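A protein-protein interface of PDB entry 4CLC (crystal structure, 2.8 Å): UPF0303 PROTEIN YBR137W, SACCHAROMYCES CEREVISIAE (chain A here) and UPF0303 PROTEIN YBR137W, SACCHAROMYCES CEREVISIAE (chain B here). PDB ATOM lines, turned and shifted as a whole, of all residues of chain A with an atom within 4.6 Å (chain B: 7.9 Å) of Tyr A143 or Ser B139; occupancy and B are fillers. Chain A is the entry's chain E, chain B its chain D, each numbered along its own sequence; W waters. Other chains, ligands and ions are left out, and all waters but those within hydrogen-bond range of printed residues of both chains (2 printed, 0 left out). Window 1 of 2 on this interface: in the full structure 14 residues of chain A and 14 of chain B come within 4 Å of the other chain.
N of Phe A34 sits at hydrogen-bond distance from O of Arg B138 (2.9 Å).
The backbone carbonyl oxygen (O) of Phe A34 sits close to the side-chain hydroxyl (OG) of Ser B139, at 3.2 Å.
O of Phe A34 lies within hydrogen-bond range of N of Asp B140, 3.1 Å away.
The side-chain hydroxyl (OG) of Ser B136 lies within hydrogen-bond range of the backbone NH (N) of Arg B138.
N of Ser B139 lies within hydrogen-bond range of OG of Ser B136 (3.2 Å).
N of Tyr B141 lies within hydrogen-bond range of OG of Ser B139.
The backbone carbonyl oxygen (O) of Ile A134 is in hydrogen-bond range of the backbone NH (N) of Tyr A143 (2.8 Å).
The side-chain hydroxyl (OG) of Ser A136 sits at hydrogen-bond distance from the side-chain hydroxyl (OH) of Tyr A143.
Water W1 lies within hydrogen-bond range of the side-chain hydroxyl (OH) of Tyr B143 (2.5 Å), the side-chain hydroxyl (OG) of Ser A136 (2.6 Å) and the side-chain hydroxyl (OH) of Tyr A143 (2.7 Å).
Water W2 bridges O of Pro B142 and O of Tyr A143.
CA of Thr A33 touches O of Arg B138, at 3.0 Å.
Phe A34 touches Tyr B141 (CD2 to CD2, 3.8 Å).
Tyr B141 touches Leu A65 (CD1 to CD1, 3.5 Å).
Pro B66 touches Pro A66 (CG to CG, 3.5 Å).
OH of Tyr A143 touches CB of Arg B138 (3.7 Å).
Tyr A143 touches Ser B139.
Ser B139 touches two residues of chain A.
Of the printed residues of chain B, Pro A66 touches Pro B66.
Of the printed residues of chain B, Thr A33 touches Arg B138 (3.0 Å).
Printed residues of chain A within 4 Å of Asp B140: Phe A34.
Printed residues of chain A within 4 Å of Pro B66: Pro A66.
Leu B31 touches none of the printed residues of chain A.
The nearest residue of chain B that does not touch Tyr A143 is Ser B136 (4.5 Å).
The nearest printed residue of chain A that does not touch Ser B139 is Thr A33 (5.2 Å).
Hydrophobic or aromatic side chains of chain B within 4 Å of the printed part of chain A: Pro B66 and Tyr B141.
Along chain B the printed residues that touch a printed residue of chain A span positions 66 to 141.
Printed residues of chain A that touch a printed residue of chain B: Thr A33, Phe A34, Leu A65, Pro A66 and Tyr A143.
Hydrophobic or aromatic side chains of chain A that line the printed part of chain B: Phe A34, Leu A65, Pro A66 and Tyr A143.
Among the printed residues, 9 pairs touch across the chains.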
ATOM      1  N   LEU A  31      17.914   3.521  -0.652  1.00  0.00           N
ATOM      2  CA  LEU A  31      17.852   4.162   0.648  1.00  0.00           C
ATOM      3  C   LEU A  31      19.191   4.804   1.022  1.00  0.00           C
ATOM      4  O   LEU A  31      20.261   4.365   0.574  1.00  0.00           O
ATOM      5  CB  LEU A  31      17.435   3.143   1.716  1.00  0.00           C
ATOM      6  CG  LEU A  31      16.365   2.122   1.316  1.00  0.00           C
ATOM      7  CD1 LEU A  31      16.286   0.978   2.323  1.00  0.00           C
ATOM      8  CD2 LEU A  31      15.008   2.780   1.183  1.00  0.00           C
ATOM      9  N   THR A  33      21.227   5.131   4.516  1.00  0.00           N
ATOM     10  CA  THR A  33      21.161   4.361   5.780  1.00  0.00           C
ATOM     11  C   THR A  33      20.398   2.996   5.744  1.00  0.00           C
ATOM     12  O   THR A  33      19.194   2.941   5.956  1.00  0.00           O
ATOM     13  CB  THR A  33      20.636   5.239   7.005  1.00  0.00           C
ATOM     14  OG1 THR A  33      20.923   4.560   8.238  1.00  0.00           O
ATOM     15  CG2 THR A  33      19.144   5.618   6.979  1.00  0.00           C
ATOM     16  N   PHE A  34      21.060   1.909   5.360  1.00  0.00           N
ATOM     17  CA  PHE A  34      20.485   0.569   5.625  1.00  0.00           C
ATOM     18  C   PHE A  34      21.009  -0.137   6.905  1.00  0.00           C
ATOM     19  O   PHE A  34      22.155  -0.597   6.942  1.00  0.00           O
ATOM     20  CB  PHE A  34      20.749  -0.338   4.420  1.00  0.00           C
ATOM     21  CG  PHE A  34      19.921  -1.593   4.390  1.00  0.00           C
ATOM     22  CD1 PHE A  34      18.607  -1.560   3.963  1.00  0.00           C
ATOM     23  CD2 PHE A  34      20.472  -2.809   4.749  1.00  0.00           C
ATOM     24  CE1 PHE A  34      17.850  -2.723   3.916  1.00  0.00           C
ATOM     25  CE2 PHE A  34      19.721  -3.971   4.707  1.00  0.00           C
ATOM     26  CZ  PHE A  34      18.408  -3.931   4.290  1.00  0.00           C
ATOM     27  N   LEU A  65      20.491 -10.274   2.642  1.00  0.00           N
ATOM     28  CA  LEU A  65      21.715  -9.668   2.127  1.00  0.00           C
ATOM     29  C   LEU A  65      22.112 -10.362   0.842  1.00  0.00           C
ATOM     30  O   LEU A  65      21.560 -11.394   0.519  1.00  0.00           O
ATOM     31  CB  LEU A  65      22.843  -9.754   3.161  1.00  0.00           C
ATOM     32  CG  LEU A  65      22.603  -8.965   4.449  1.00  0.00           C
ATOM     33  CD1 LEU A  65      23.884  -8.843   5.225  1.00  0.00           C
ATOM     34  CD2 LEU A  65      21.993  -7.586   4.171  1.00  0.00           C
ATOM     35  N   PRO A  66      23.051  -9.785   0.082  1.00  0.00           N
ATOM     36  CA  PRO A  66      23.458 -10.472  -1.149  1.00  0.00           C
ATOM     37  C   PRO A  66      24.199 -11.775  -0.907  1.00  0.00           C
ATOM     38  O   PRO A  66      24.281 -12.582  -1.810  1.00  0.00           O
ATOM     39  CB  PRO A  66      24.362  -9.444  -1.842  1.00  0.00           C
ATOM     40  CG  PRO A  66      24.604  -8.392  -0.860  1.00  0.00           C
ATOM     41  CD  PRO A  66      23.476  -8.379   0.079  1.00  0.00           C
ATOM     42  N   ILE A 134      17.315  -3.711  -3.326  1.00  0.00           N
ATOM     43  CA  ILE A 134      17.335  -2.491  -2.545  1.00  0.00           C
ATOM     44  C   ILE A 134      18.656  -1.780  -2.828  1.00  0.00           C
ATOM     45  O   ILE A 134      19.730  -2.219  -2.390  1.00  0.00           O
ATOM     46  CB  ILE A 134      17.203  -2.811  -1.061  1.00  0.00           C
ATOM     47  CG1 ILE A 134      15.980  -3.701  -0.846  1.00  0.00           C
ATOM     48  CG2 ILE A 134      17.179  -1.548  -0.222  1.00  0.00           C
ATOM     49  CD1 ILE A 134      15.777  -4.100   0.563  1.00  0.00           C
ATOM     50  N   GLN A 135      18.563  -0.679  -3.572  1.00  0.00           N
ATOM     51  CA  GLN A 135      19.747   0.003  -4.082  1.00  0.00           C
ATOM     52  C   GLN A 135      20.372   0.901  -3.026  1.00  0.00           C
ATOM     53  O   GLN A 135      19.718   1.345  -2.081  1.00  0.00           O
ATOM     54  CB  GLN A 135      19.414   0.818  -5.331  1.00  0.00           C
ATOM     55  CG  GLN A 135      18.820   0.036  -6.471  1.00  0.00           C
ATOM     56  CD  GLN A 135      19.769  -0.998  -7.034  1.00  0.00           C
ATOM     57  OE1 GLN A 135      20.950  -1.047  -6.666  1.00  0.00           O
ATOM     58  NE2 GLN A 135      19.265  -1.830  -7.947  1.00  0.00           N
ATOM     59  N   SER A 136      21.658   1.147  -3.178  1.00  0.00           N
ATOM     60  CA  SER A 136      22.315   2.118  -2.333  1.00  0.00           C
ATOM     61  C   SER A 136      22.575   3.377  -3.142  1.00  0.00           C
ATOM     62  O   SER A 136      23.080   3.325  -4.268  1.00  0.00           O
ATOM     63  CB  SER A 136      23.617   1.549  -1.768  1.00  0.00           C
ATOM     64  OG  SER A 136      24.384   2.549  -1.113  1.00  0.00           O
ATOM     65  N   TYR A 141      26.125  -0.916  -6.169  1.00  0.00           N
ATOM     66  CA  TYR A 141      25.744  -2.284  -5.844  1.00  0.00           C
ATOM     67  C   TYR A 141      24.745  -2.319  -4.687  1.00  0.00           C
ATOM     68  O   TYR A 141      24.842  -1.520  -3.752  1.00  0.00           O
ATOM     69  CB  TYR A 141      26.990  -3.093  -5.533  1.00  0.00           C
ATOM     70  CG  TYR A 141      28.008  -2.949  -6.615  1.00  0.00           C
ATOM     71  CD1 TYR A 141      27.756  -3.445  -7.884  1.00  0.00           C
ATOM     72  CD2 TYR A 141      29.216  -2.286  -6.386  1.00  0.00           C
ATOM     73  CE1 TYR A 141      28.678  -3.304  -8.892  1.00  0.00           C
ATOM     74  CE2 TYR A 141      30.148  -2.133  -7.396  1.00  0.00           C
ATOM     75  CZ  TYR A 141      29.870  -2.649  -8.647  1.00  0.00           C
ATOM     76  OH  TYR A 141      30.766  -2.516  -9.679  1.00  0.00           O
ATOM     77  N   PRO A 142      23.777  -3.252  -4.751  1.00  0.00           N
ATOM     78  CA  PRO A 142      22.613  -3.239  -3.862  1.00  0.00           C
ATOM     79  C   PRO A 142      22.955  -3.536  -2.414  1.00  0.00           C
ATOM     80  O   PRO A 142      23.831  -4.358  -2.159  1.00  0.00           O
ATOM     81  CB  PRO A 142      21.728  -4.347  -4.439  1.00  0.00           C
ATOM     82  CG  PRO A 142      22.673  -5.275  -5.063  1.00  0.00           C
ATOM     83  CD  PRO A 142      23.745  -4.407  -5.664  1.00  0.00           C
ATOM     84  N   TYR A 143      22.264  -2.874  -1.488  1.00  0.00           N
ATOM     85  CA  TYR A 143      22.374  -3.186  -0.069  1.00  0.00           C
ATOM     86  C   TYR A 143      21.978  -4.625   0.167  1.00  0.00           C
ATOM     87  O   TYR A 143      22.732  -5.417   0.750  1.00  0.00           O
ATOM     88  CB  TYR A 143      21.476  -2.272   0.772  1.00  0.00           C
ATOM     89  CG  TYR A 143      22.035  -0.888   1.056  1.00  0.00           C
ATOM     90  CD1 TYR A 143      23.383  -0.687   1.268  1.00  0.00           C
ATOM     91  CD2 TYR A 143      21.198   0.211   1.110  1.00  0.00           C
ATOM     92  CE1 TYR A 143      23.871   0.566   1.527  1.00  0.00           C
ATOM     93  CE2 TYR A 143      21.672   1.458   1.369  1.00  0.00           C
ATOM     94  CZ  TYR A 143      23.005   1.641   1.577  1.00  0.00           C
ATOM     95  OH  TYR A 143      23.476   2.920   1.836  1.00  0.00           O
ATOM     96  N   ALA A 144      20.781  -4.949  -0.315  1.00  0.00           N
ATOM     97  CA  ALA A 144      20.140  -6.227  -0.048  1.00  0.00           C
ATOM     98  C   ALA A 144      19.008  -6.460  -1.042  1.00  0.00           C
ATOM     99  O   ALA A 144      18.770  -5.641  -1.926  1.00  0.00           O
ATOM    100  CB  ALA A 144      19.617  -6.264   1.385  1.00  0.00           C
ATOM    101  N   PHE B  30      36.292   1.587   6.121  1.00  0.00           N
ATOM    102  CA  PHE B  30      35.009   1.854   5.519  1.00  0.00           C
ATOM    103  C   PHE B  30      35.073   3.001   4.535  1.00  0.00           C
ATOM    104  O   PHE B  30      35.836   3.940   4.701  1.00  0.00           O
ATOM    105  CB  PHE B  30      33.954   2.119   6.598  1.00  0.00           C
ATOM    106  CG  PHE B  30      33.997   3.494   7.197  1.00  0.00           C
ATOM    107  CD1 PHE B  30      34.784   3.757   8.307  1.00  0.00           C
ATOM    108  CD2 PHE B  30      33.213   4.518   6.681  1.00  0.00           C
ATOM    109  CE1 PHE B  30      34.808   5.025   8.881  1.00  0.00           C
ATOM    110  CE2 PHE B  30      33.231   5.787   7.247  1.00  0.00           C
ATOM    111  CZ  PHE B  30      34.029   6.039   8.353  1.00  0.00           C
ATOM    112  N   LEU B  31      34.241   2.904   3.511  1.00  0.00           N
ATOM    113  CA  LEU B  31      34.202   3.876   2.448  1.00  0.00           C
ATOM    114  C   LEU B  31      32.841   4.522   2.488  1.00  0.00           C
ATOM    115  O   LEU B  31      31.900   3.956   3.040  1.00  0.00           O
ATOM    116  CB  LEU B  31      34.462   3.207   1.107  1.00  0.00           C
ATOM    117  CG  LEU B  31      35.668   2.273   1.196  1.00  0.00           C
ATOM    118  CD1 LEU B  31      35.823   1.402  -0.053  1.00  0.00           C
ATOM    119  CD2 LEU B  31      36.901   3.110   1.435  1.00  0.00           C
ATOM    120  N   SER B  32      32.737   5.723   1.946  1.00  0.00           N
ATOM    121  CA  SER B  32      31.446   6.374   1.895  1.00  0.00           C
ATOM    122  C   SER B  32      30.788   6.123   0.561  1.00  0.00           C
ATOM    123  O   SER B  32      29.651   6.532   0.363  1.00  0.00           O
ATOM    124  CB  SER B  32      31.581   7.880   2.148  1.00  0.00           C
ATOM    125  OG  SER B  32      31.790   8.154   3.532  1.00  0.00           O
ATOM    126  N   PRO B  66      29.674  -9.507  -1.587  1.00  0.00           N
ATOM    127  CA  PRO B  66      29.293 -10.633  -0.734  1.00  0.00           C
ATOM    128  C   PRO B  66      28.593 -11.737  -1.494  1.00  0.00           C
ATOM    129  O   PRO B  66      28.552 -12.863  -1.007  1.00  0.00           O
ATOM    130  CB  PRO B  66      28.344 -10.002   0.286  1.00  0.00           C
ATOM    131  CG  PRO B  66      28.012  -8.669  -0.250  1.00  0.00           C
ATOM    132  CD  PRO B  66      29.147  -8.236  -1.071  1.00  0.00           C
ATOM    133  N   ILE B 134      35.014  -4.887   3.642  1.00  0.00           N
ATOM    134  CA  ILE B 134      34.945  -3.463   3.379  1.00  0.00           C
ATOM    135  C   ILE B 134      33.614  -2.941   3.890  1.00  0.00           C
ATOM    136  O   ILE B 134      32.568  -3.192   3.287  1.00  0.00           O
ATOM    137  CB  ILE B 134      35.065  -3.141   1.875  1.00  0.00           C
ATOM    138  CG1 ILE B 134      36.355  -3.697   1.286  1.00  0.00           C
ATOM    139  CG2 ILE B 134      34.996  -1.638   1.653  1.00  0.00           C
ATOM    140  CD1 ILE B 134      36.509  -3.377  -0.182  1.00  0.00           C
ATOM    141  N   GLN B 135      33.660  -2.190   4.985  1.00  0.00           N
ATOM    142  CA  GLN B 135      32.451  -1.699   5.650  1.00  0.00           C
ATOM    143  C   GLN B 135      31.868  -0.474   4.977  1.00  0.00           C
ATOM    144  O   GLN B 135      32.585   0.277   4.319  1.00  0.00           O
ATOM    145  CB  GLN B 135      32.746  -1.377   7.108  1.00  0.00           C
ATOM    146  CG  GLN B 135      31.897  -2.165   8.051  1.00  0.00           C
ATOM    147  CD  GLN B 135      32.271  -3.614   8.064  1.00  0.00           C
ATOM    148  OE1 GLN B 135      33.432  -3.966   8.295  1.00  0.00           O
ATOM    149  NE2 GLN B 135      31.294  -4.478   7.807  1.00  0.00           N
ATOM    150  N   SER B 136      30.565  -0.276   5.146  1.00  0.00           N
ATOM    151  CA  SER B 136      29.888   0.892   4.589  1.00  0.00           C
ATOM    152  C   SER B 136      29.481   1.842   5.696  1.00  0.00           C
ATOM    153  O   SER B 136      28.976   1.419   6.743  1.00  0.00           O
ATOM    154  CB  SER B 136      28.655   0.484   3.792  1.00  0.00           C
ATOM    155  OG  SER B 136      27.670   1.504   3.817  1.00  0.00           O
ATOM    156  N   GLU B 137      29.697   3.126   5.464  1.00  0.00           N
ATOM    157  CA  GLU B 137      29.338   4.128   6.438  1.00  0.00           C
ATOM    158  C   GLU B 137      27.846   4.108   6.708  1.00  0.00           C
ATOM    159  O   GLU B 137      27.421   4.169   7.851  1.00  0.00           O
ATOM    160  CB  GLU B 137      29.768   5.493   5.962  1.00  0.00           C
ATOM    161  N   ARG B 138      27.042   4.008   5.662  1.00  0.00           N
ATOM    162  CA  ARG B 138      25.608   4.181   5.830  1.00  0.00           C
ATOM    163  C   ARG B 138      24.896   2.868   6.169  1.00  0.00           C
ATOM    164  O   ARG B 138      23.677   2.827   6.305  1.00  0.00           O
ATOM    165  CB  ARG B 138      25.009   4.806   4.572  1.00  0.00           C
ATOM    166  N   SER B 139      25.650   1.791   6.323  1.00  0.00           N
ATOM    167  CA  SER B 139      25.023   0.483   6.494  1.00  0.00           C
ATOM    168  C   SER B 139      25.685  -0.349   7.588  1.00  0.00           C
ATOM    169  O   SER B 139      26.892  -0.225   7.816  1.00  0.00           O
ATOM    170  CB  SER B 139      25.045  -0.277   5.153  1.00  0.00           C
ATOM    171  OG  SER B 139      24.636  -1.632   5.289  1.00  0.00           O
ATOM    172  N   ASP B 140      24.896  -1.200   8.249  1.00  0.00           N
ATOM    173  CA  ASP B 140      25.440  -2.184   9.195  1.00  0.00           C
ATOM    174  C   ASP B 140      26.123  -3.330   8.455  1.00  0.00           C
ATOM    175  O   ASP B 140      26.829  -4.147   9.053  1.00  0.00           O
ATOM    176  CB  ASP B 140      24.358  -2.774  10.107  1.00  0.00           C
ATOM    177  CG  ASP B 140      23.646  -1.727  10.954  1.00  0.00           C
ATOM    178  OD1 ASP B 140      24.167  -0.594  11.090  1.00  0.00           O
ATOM    179  OD2 ASP B 140      22.561  -2.061  11.497  1.00  0.00           O
ATOM    180  N   TYR B 141      25.926  -3.396   7.150  1.00  0.00           N
ATOM    181  CA  TYR B 141      26.426  -4.540   6.417  1.00  0.00           C
ATOM    182  C   TYR B 141      27.445  -4.111   5.383  1.00  0.00           C
ATOM    183  O   TYR B 141      27.291  -3.063   4.751  1.00  0.00           O
ATOM    184  CB  TYR B 141      25.247  -5.275   5.797  1.00  0.00           C
ATOM    185  CG  TYR B 141      24.167  -5.491   6.833  1.00  0.00           C
ATOM    186  CD1 TYR B 141      24.272  -6.522   7.761  1.00  0.00           C
ATOM    187  CD2 TYR B 141      23.063  -4.637   6.916  1.00  0.00           C
ATOM    188  CE1 TYR B 141      23.303  -6.712   8.722  1.00  0.00           C
ATOM    189  CE2 TYR B 141      22.088  -4.828   7.875  1.00  0.00           C
ATOM    190  CZ  TYR B 141      22.217  -5.864   8.777  1.00  0.00           C
ATOM    191  OH  TYR B 141      21.265  -6.065   9.737  1.00  0.00           O
ATOM    192  N   PRO B 142      28.488  -4.933   5.207  1.00  0.00           N
ATOM    193  CA  PRO B 142      29.679  -4.625   4.415  1.00  0.00           C
ATOM    194  C   PRO B 142      29.398  -4.433   2.927  1.00  0.00           C
ATOM    195  O   PRO B 142      28.543  -5.127   2.366  1.00  0.00           O
ATOM    196  CB  PRO B 142      30.570  -5.847   4.637  1.00  0.00           C
ATOM    197  CG  PRO B 142      29.656  -6.915   5.017  1.00  0.00           C
ATOM    198  CD  PRO B 142      28.561  -6.280   5.790  1.00  0.00           C
ATOM    199  N   TYR B 143      30.112  -3.486   2.315  1.00  0.00           N
ATOM    200  CA  TYR B 143      30.091  -3.287   0.867  1.00  0.00           C
ATOM    201  C   TYR B 143      30.594  -4.533   0.148  1.00  0.00           C
ATOM    202  O   TYR B 143      29.996  -5.007  -0.816  1.00  0.00           O
ATOM    203  CB  TYR B 143      30.965  -2.088   0.456  1.00  0.00           C
ATOM    204  CG  TYR B 143      30.290  -0.738   0.510  1.00  0.00           C
ATOM    205  CD1 TYR B 143      28.967  -0.598   0.144  1.00  0.00           C
ATOM    206  CD2 TYR B 143      30.986   0.404   0.921  1.00  0.00           C
ATOM    207  CE1 TYR B 143      28.337   0.634   0.189  1.00  0.00           C
ATOM    208  CE2 TYR B 143      30.366   1.637   0.971  1.00  0.00           C
ATOM    209  CZ  TYR B 143      29.040   1.741   0.597  1.00  0.00           C
ATOM    210  OH  TYR B 143      28.384   2.941   0.628  1.00  0.00           O
HETATM  211  O   HOH W   1      25.917   3.327   0.881  1.00  0.00           O
HETATM  212  O   HOH W   2      25.590  -6.239   2.430  1.00  0.00           O
